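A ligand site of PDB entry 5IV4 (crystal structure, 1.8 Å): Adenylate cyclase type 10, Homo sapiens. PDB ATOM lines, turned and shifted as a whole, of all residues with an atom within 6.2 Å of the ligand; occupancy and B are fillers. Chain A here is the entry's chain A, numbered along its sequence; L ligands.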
ATOM      1  N   PHE A  45     -17.554  16.643 -26.352  1.00  0.00           N
ATOM      2  CA  PHE A  45     -17.258  17.501 -25.110  1.00  0.00           C
ATOM      3  C   PHE A  45     -18.009  18.740 -25.225  1.00  0.00           C
ATOM      4  O   PHE A  45     -17.965  19.424 -26.285  1.00  0.00           O
ATOM      5  CB  PHE A  45     -15.767  17.767 -24.958  1.00  0.00           C
ATOM      6  CG  PHE A  45     -15.402  18.409 -23.640  1.00  0.00           C
ATOM      7  CD1 PHE A  45     -15.820  17.811 -22.441  1.00  0.00           C
ATOM      8  CD2 PHE A  45     -14.587  19.500 -23.563  1.00  0.00           C
ATOM      9  CE1 PHE A  45     -15.586  18.398 -21.227  1.00  0.00           C
ATOM     10  CE2 PHE A  45     -14.278  20.087 -22.327  1.00  0.00           C
ATOM     11  CZ  PHE A  45     -14.730  19.499 -21.169  1.00  0.00           C
ATOM     12  N   LEU A  94     -20.012  10.152 -19.812  1.00  0.00           N
ATOM     13  CA  LEU A  94     -18.887   9.546 -19.062  1.00  0.00           C
ATOM     14  C   LEU A  94     -18.598  10.207 -17.720  1.00  0.00           C
ATOM     15  O   LEU A  94     -18.530   9.501 -16.683  1.00  0.00           O
ATOM     16  CB  LEU A  94     -17.608   9.511 -19.870  1.00  0.00           C
ATOM     17  CG  LEU A  94     -17.660   8.658 -21.135  1.00  0.00           C
ATOM     18  CD1 LEU A  94     -16.281   8.732 -21.819  1.00  0.00           C
ATOM     19  CD2 LEU A  94     -18.101   7.267 -20.887  1.00  0.00           C
ATOM     20  N   LYS A  95     -18.503  11.538 -17.719  1.00  0.00           N
ATOM     21  CA  LYS A  95     -18.148  12.329 -16.524  1.00  0.00           C
ATOM     22  C   LYS A  95     -18.635  13.730 -16.697  1.00  0.00           C
ATOM     23  O   LYS A  95     -18.704  14.235 -17.840  1.00  0.00           O
ATOM     24  CB  LYS A  95     -16.619  12.385 -16.289  1.00  0.00           C
ATOM     25  CG  LYS A  95     -16.120  11.504 -15.267  1.00  0.00           C
ATOM     26  CD  LYS A  95     -14.629  11.632 -14.937  1.00  0.00           C
ATOM     27  CE  LYS A  95     -14.159  10.225 -14.587  1.00  0.00           C
ATOM     28  NZ  LYS A  95     -12.802  10.195 -14.004  1.00  0.00           N
ATOM     29  N   PHE A  96     -18.965  14.370 -15.578  1.00  0.00           N
ATOM     30  CA  PHE A  96     -19.239  15.785 -15.529  1.00  0.00           C
ATOM     31  C   PHE A  96     -18.105  16.497 -14.813  1.00  0.00           C
ATOM     32  O   PHE A  96     -17.410  15.934 -13.972  1.00  0.00           O
ATOM     33  CB  PHE A  96     -20.479  16.064 -14.718  1.00  0.00           C
ATOM     34  CG  PHE A  96     -21.721  15.533 -15.271  1.00  0.00           C
ATOM     35  CD1 PHE A  96     -22.063  14.225 -15.029  1.00  0.00           C
ATOM     36  CD2 PHE A  96     -22.657  16.356 -15.954  1.00  0.00           C
ATOM     37  CE1 PHE A  96     -23.271  13.682 -15.401  1.00  0.00           C
ATOM     38  CE2 PHE A  96     -23.856  15.763 -16.343  1.00  0.00           C
ATOM     39  CZ  PHE A  96     -24.165  14.480 -16.081  1.00  0.00           C
ATOM     40  N   ALA A  97     -17.863  17.752 -15.171  1.00  0.00           N
ATOM     41  CA  ALA A  97     -16.941  18.600 -14.419  1.00  0.00           C
ATOM     42  C   ALA A  97     -17.521  19.972 -14.468  1.00  0.00           C
ATOM     43  O   ALA A  97     -17.559  20.591 -15.527  1.00  0.00           O
ATOM     44  CB  ALA A  97     -15.570  18.568 -15.017  1.00  0.00           C
ATOM     45  N   ALA A 100     -19.497  21.227 -17.548  1.00  0.00           N
ATOM     46  CA  ALA A 100     -19.010  20.522 -18.735  1.00  0.00           C
ATOM     47  C   ALA A 100     -19.307  19.039 -18.599  1.00  0.00           C
ATOM     48  O   ALA A 100     -19.441  18.548 -17.456  1.00  0.00           O
ATOM     49  CB  ALA A 100     -17.526  20.733 -18.903  1.00  0.00           C
ATOM     50  N   LEU A 101     -19.453  18.330 -19.739  1.00  0.00           N
ATOM     51  CA  LEU A 101     -19.564  16.913 -19.716  1.00  0.00           C
ATOM     52  C   LEU A 101     -18.957  16.295 -20.975  1.00  0.00           C
ATOM     53  O   LEU A 101     -18.927  16.958 -22.007  1.00  0.00           O
ATOM     54  CB  LEU A 101     -21.008  16.409 -19.455  1.00  0.00           C
ATOM     55  CG  LEU A 101     -21.999  16.773 -20.608  1.00  0.00           C
ATOM     56  CD1 LEU A 101     -22.050  15.756 -21.738  1.00  0.00           C
ATOM     57  CD2 LEU A 101     -23.391  16.829 -20.040  1.00  0.00           C
ATOM     58  N   LEU A 102     -18.456  15.072 -20.839  1.00  0.00           N
ATOM     59  CA  LEU A 102     -17.907  14.267 -21.927  1.00  0.00           C
ATOM     60  C   LEU A 102     -18.786  13.116 -22.155  1.00  0.00           C
ATOM     61  O   LEU A 102     -19.139  12.415 -21.211  1.00  0.00           O
ATOM     62  CB  LEU A 102     -16.506  13.812 -21.491  1.00  0.00           C
ATOM     63  CG  LEU A 102     -15.704  12.966 -22.520  1.00  0.00           C
ATOM     64  CD1 LEU A 102     -15.436  13.782 -23.789  1.00  0.00           C
ATOM     65  CD2 LEU A 102     -14.414  12.368 -21.926  1.00  0.00           C
ATOM     66  N   PHE A 165     -12.105   5.832 -13.123  1.00  0.00           N
ATOM     67  CA  PHE A 165     -11.821   5.539 -14.536  1.00  0.00           C
ATOM     68  C   PHE A 165     -11.525   6.777 -15.356  1.00  0.00           C
ATOM     69  O   PHE A 165     -11.881   7.920 -14.968  1.00  0.00           O
ATOM     70  CB  PHE A 165     -12.926   4.747 -15.199  1.00  0.00           C
ATOM     71  CG  PHE A 165     -14.135   5.572 -15.589  1.00  0.00           C
ATOM     72  CD1 PHE A 165     -15.056   5.861 -14.679  1.00  0.00           C
ATOM     73  CD2 PHE A 165     -14.262   6.068 -16.863  1.00  0.00           C
ATOM     74  CE1 PHE A 165     -16.146   6.695 -14.979  1.00  0.00           C
ATOM     75  CE2 PHE A 165     -15.366   6.822 -17.180  1.00  0.00           C
ATOM     76  CZ  PHE A 165     -16.250   7.152 -16.234  1.00  0.00           C
ATOM     77  N   LEU A 166     -10.849   6.538 -16.496  1.00  0.00           N
ATOM     78  CA  LEU A 166     -10.548   7.576 -17.476  1.00  0.00           C
ATOM     79  C   LEU A 166     -10.646   6.989 -18.848  1.00  0.00           C
ATOM     80  O   LEU A 166     -10.422   5.812 -18.994  1.00  0.00           O
ATOM     81  CB  LEU A 166      -9.072   8.046 -17.385  1.00  0.00           C
ATOM     82  CG  LEU A 166      -8.800   8.777 -16.089  1.00  0.00           C
ATOM     83  CD1 LEU A 166      -7.327   8.825 -15.863  1.00  0.00           C
ATOM     84  CD2 LEU A 166      -9.379  10.170 -16.169  1.00  0.00           C
ATOM     85  N   VAL A 167     -10.965   7.792 -19.849  1.00  0.00           N
ATOM     86  CA  VAL A 167     -10.703   7.401 -21.243  1.00  0.00           C
ATOM     87  C   VAL A 167      -9.473   8.196 -21.741  1.00  0.00           C
ATOM     88  O   VAL A 167      -9.194   9.310 -21.315  1.00  0.00           O
ATOM     89  CB  VAL A 167     -11.918   7.576 -22.196  1.00  0.00           C
ATOM     90  CG1 VAL A 167     -12.950   6.578 -21.919  1.00  0.00           C
ATOM     91  CG2 VAL A 167     -12.422   8.973 -22.155  1.00  0.00           C
ATOM     92  N   ILE A 168      -8.695   7.552 -22.584  1.00  0.00           N
ATOM     93  CA  ILE A 168      -7.358   7.988 -23.002  1.00  0.00           C
ATOM     94  C   ILE A 168      -7.176   7.794 -24.498  1.00  0.00           C
ATOM     95  O   ILE A 168      -7.678   6.884 -25.026  1.00  0.00           O
ATOM     96  CB  ILE A 168      -6.287   7.160 -22.175  1.00  0.00           C
ATOM     97  CG1 ILE A 168      -6.330   7.672 -20.731  1.00  0.00           C
ATOM     98  CG2 ILE A 168      -4.862   7.341 -22.645  1.00  0.00           C
ATOM     99  CD1 ILE A 168      -5.453   6.886 -19.765  1.00  0.00           C
ATOM    100  N   VAL A 172      -9.401  11.385 -27.473  1.00  0.00           N
ATOM    101  CA  VAL A 172      -9.654  12.116 -26.258  1.00  0.00           C
ATOM    102  C   VAL A 172      -8.977  13.506 -26.259  1.00  0.00           C
ATOM    103  O   VAL A 172      -9.614  14.524 -26.039  1.00  0.00           O
ATOM    104  CB  VAL A 172      -9.252  11.262 -25.050  1.00  0.00           C
ATOM    105  CG1 VAL A 172      -9.543  12.062 -23.778  1.00  0.00           C
ATOM    106  CG2 VAL A 172     -10.059   9.991 -25.030  1.00  0.00           C
ATOM    107  N   ASP A 173      -7.685  13.557 -26.572  1.00  0.00           N
ATOM    108  CA  ASP A 173      -6.950  14.852 -26.724  1.00  0.00           C
ATOM    109  C   ASP A 173      -7.575  15.705 -27.774  1.00  0.00           C
ATOM    110  O   ASP A 173      -7.773  16.878 -27.545  1.00  0.00           O
ATOM    111  CB  ASP A 173      -5.469  14.650 -27.022  1.00  0.00           C
ATOM    112  CG  ASP A 173      -4.763  13.796 -25.978  1.00  0.00           C
ATOM    113  OD1 ASP A 173      -5.254  13.639 -24.830  1.00  0.00           O
ATOM    114  OD2 ASP A 173      -3.755  13.189 -26.303  1.00  0.00           O
ATOM    115  N   VAL A 175     -10.740  15.785 -28.829  1.00  0.00           N
ATOM    116  CA  VAL A 175     -12.041  16.365 -28.528  1.00  0.00           C
ATOM    117  C   VAL A 175     -11.868  17.572 -27.627  1.00  0.00           C
ATOM    118  O   VAL A 175     -12.644  18.549 -27.674  1.00  0.00           O
ATOM    119  CB  VAL A 175     -13.055  15.305 -28.007  1.00  0.00           C
ATOM    120  CG1 VAL A 175     -12.816  14.927 -26.556  1.00  0.00           C
ATOM    121  CG2 VAL A 175     -14.448  15.774 -28.175  1.00  0.00           C
ATOM    122  N   ARG A 176     -10.890  17.455 -26.737  1.00  0.00           N
ATOM    123  CA  ARG A 176     -10.618  18.573 -25.843  1.00  0.00           C
ATOM    124  C   ARG A 176     -10.146  19.771 -26.712  1.00  0.00           C
ATOM    125  O   ARG A 176     -10.568  20.910 -26.529  1.00  0.00           O
ATOM    126  CB  ARG A 176      -9.554  18.179 -24.833  1.00  0.00           C
ATOM    127  CG  ARG A 176      -9.735  18.730 -23.416  1.00  0.00           C
ATOM    128  CD  ARG A 176      -9.190  20.107 -23.206  1.00  0.00           C
ATOM    129  NE  ARG A 176      -7.885  20.275 -23.864  1.00  0.00           N
ATOM    130  CZ  ARG A 176      -7.209  21.423 -23.969  1.00  0.00           C
ATOM    131  NH1 ARG A 176      -6.033  21.412 -24.598  1.00  0.00           N
ATOM    132  NH2 ARG A 176      -7.654  22.543 -23.412  1.00  0.00           N
ATOM    133  N   LYS A 334     -12.462  14.478  -8.582  1.00  0.00           N
ATOM    134  CA  LYS A 334     -12.556  14.154  -9.996  1.00  0.00           C
ATOM    135  C   LYS A 334     -11.150  13.839 -10.536  1.00  0.00           C
ATOM    136  O   LYS A 334     -10.205  14.315  -9.996  1.00  0.00           O
ATOM    137  CB  LYS A 334     -13.171  15.363 -10.753  1.00  0.00           C
ATOM    138  CG  LYS A 334     -13.984  15.053 -12.014  1.00  0.00           C
ATOM    139  CD  LYS A 334     -15.275  14.288 -11.772  1.00  0.00           C
ATOM    140  CE  LYS A 334     -16.367  15.061 -11.058  1.00  0.00           C
ATOM    141  NZ  LYS A 334     -17.570  14.152 -11.114  1.00  0.00           N
ATOM    142  N   VAL A 335     -11.038  12.961 -11.557  1.00  0.00           N
ATOM    143  CA  VAL A 335      -9.782  12.698 -12.233  1.00  0.00           C
ATOM    144  C   VAL A 335     -10.001  12.913 -13.739  1.00  0.00           C
ATOM    145  O   VAL A 335     -11.066  12.552 -14.240  1.00  0.00           O
ATOM    146  CB  VAL A 335      -9.289  11.304 -11.953  1.00  0.00           C
ATOM    147  CG1 VAL A 335      -7.882  11.136 -12.473  1.00  0.00           C
ATOM    148  CG2 VAL A 335      -9.305  10.966 -10.421  1.00  0.00           C
ATOM    149  N   PHE A 336      -9.033  13.575 -14.390  1.00  0.00           N
ATOM    150  CA  PHE A 336      -9.040  14.041 -15.791  1.00  0.00           C
ATOM    151  C   PHE A 336      -7.763  13.617 -16.460  1.00  0.00           C
ATOM    152  O   PHE A 336      -6.753  13.465 -15.797  1.00  0.00           O
ATOM    153  CB  PHE A 336      -9.059  15.562 -15.865  1.00  0.00           C
ATOM    154  CG  PHE A 336     -10.093  16.198 -15.039  1.00  0.00           C
ATOM    155  CD1 PHE A 336     -11.396  16.092 -15.394  1.00  0.00           C
ATOM    156  CD2 PHE A 336      -9.782  16.824 -13.841  1.00  0.00           C
ATOM    157  CE1 PHE A 336     -12.419  16.682 -14.601  1.00  0.00           C
ATOM    158  CE2 PHE A 336     -10.772  17.402 -13.068  1.00  0.00           C
ATOM    159  CZ  PHE A 336     -12.079  17.380 -13.458  1.00  0.00           C
ATOM    160  N   MET A 337      -7.808  13.400 -17.775  1.00  0.00           N
ATOM    161  CA  MET A 337      -6.564  13.164 -18.526  1.00  0.00           C
ATOM    162  C   MET A 337      -6.691  13.648 -19.974  1.00  0.00           C
ATOM    163  O   MET A 337      -7.619  13.293 -20.674  1.00  0.00           O
ATOM    164  CB  MET A 337      -6.107  11.699 -18.565  1.00  0.00           C
ATOM    165  CG  MET A 337      -4.710  11.607 -19.226  1.00  0.00           C
ATOM    166  SD  MET A 337      -3.882  10.132 -18.770  1.00  0.00           S
ATOM    167  CE  MET A 337      -2.274  10.724 -19.374  1.00  0.00           C
ATOM    168  N   PHE A 338      -5.762  14.494 -20.373  1.00  0.00           N
ATOM    169  CA  PHE A 338      -5.657  14.918 -21.766  1.00  0.00           C
ATOM    170  C   PHE A 338      -4.202  15.438 -21.978  1.00  0.00           C
ATOM    171  O   PHE A 338      -3.525  15.837 -21.011  1.00  0.00           O
ATOM    172  CB  PHE A 338      -6.695  15.919 -22.176  1.00  0.00           C
ATOM    173  CG  PHE A 338      -6.865  17.107 -21.266  1.00  0.00           C
ATOM    174  CD1 PHE A 338      -6.076  18.242 -21.398  1.00  0.00           C
ATOM    175  CD2 PHE A 338      -7.910  17.095 -20.308  1.00  0.00           C
ATOM    176  CE1 PHE A 338      -6.276  19.339 -20.566  1.00  0.00           C
ATOM    177  CE2 PHE A 338      -8.132  18.216 -19.505  1.00  0.00           C
ATOM    178  CZ  PHE A 338      -7.282  19.318 -19.620  1.00  0.00           C
HETATM  179  C1  LIG L   1     -12.456  16.606 -21.403  1.00  0.00           C
HETATM  180  C2  LIG L   1     -12.287  16.385 -22.744  1.00  0.00           C
HETATM  181  C3  LIG L   1     -11.510  15.381 -23.142  1.00  0.00           C
HETATM  182  S1  LIG L   1     -10.826  14.699 -21.730  1.00  0.00           S
HETATM  183  C4  LIG L   1     -11.655  15.771 -20.734  1.00  0.00           C
HETATM  184  C5  LIG L   1     -11.551  15.697 -19.175  1.00  0.00           C
HETATM  185  N1  LIG L   1     -12.480  14.757 -18.623  1.00  0.00           N
HETATM  186  C6  LIG L   1     -13.854  15.239 -18.607  1.00  0.00           C
HETATM  187  C7  LIG L   1     -14.528  15.306 -17.205  1.00  0.00           C
HETATM  188  C8  LIG L   1     -14.105  16.557 -18.004  1.00  0.00           C
HETATM  189  C9  LIG L   1     -12.229  13.470 -18.681  1.00  0.00           C
HETATM  190  N2  LIG L   1     -11.012  13.078 -19.026  1.00  0.00           N
HETATM  191  C10 LIG L   1     -13.193  12.465 -18.488  1.00  0.00           C
HETATM  192  C11 LIG L   1     -12.889  11.140 -18.660  1.00  0.00           C
HETATM  193 CL1  LIG L   1     -13.931   9.725 -18.382  1.00  0.00          CL
HETATM  194  N3  LIG L   1     -11.659  10.836 -19.053  1.00  0.00           N
HETATM  195  C12 LIG L   1     -10.774  11.814 -19.258  1.00  0.00           C
HETATM  196  N4  LIG L   1      -9.591  11.517 -19.733  1.00  0.00           N
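N of Met 337 sits at hydrogen-bond distance from N2 of the ligand, 3.5 Å away. N4 of the ligand sits at hydrogen-bond distance from O of Met 337 (2.8 Å). O of Val 167 lies within hydrogen-bond range of N4 of the ligand, at 2.7 Å. N3 of the ligand is in hydrogen-bond range of N of Val 167 (3.2 Å).
The backbone carbonyl oxygen of Leu 102 lies within hydrogen-bond range of the backbone NH of Leu 94 (2.8 Å). N of Leu 102 lies within hydrogen-bond range of O of Lys 95 (3.1 Å). O of Phe 165 lies within hydrogen-bond range of NZ of Lys 95 (2.6 Å). NZ of Lys 95 sits at hydrogen-bond distance from O of Val 335 (2.9 Å).
Phe 45 touches the ligand. CB of Leu 94 touches CL1 of the ligand (3.97 Å). Lys 95 touches the ligand (CB to C7, 3.7 Å). Ala 97 touches the ligand. CD2 of Leu 102 touches C10 of the ligand, at 3.6 Å. Phe 165 touches the ligand. Leu 166 touches the ligand. Val 172 touches the ligand. Val 175 touches the ligand. CG of Arg 176 touches C2 of the ligand (3.5 Å). CE1 of Phe 336 touches C7 of the ligand (3.6 Å). Phe 338 touches the ligand (CD2 to C4, 3.99 Å). Within 4 Å of the ligand: Phe 45, Leu 94, Lys 95, Ala 97, Leu 102, Phe 165, Leu 166, Val 167, Val 172, Val 175, Arg 176, Phe 336, Met 337 and Phe 338. Along chain A the residues within 4 Å of the ligand span positions 45 to 338. The nearest printed residue that does not touch the ligand is Phe 96 (4.4 Å).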
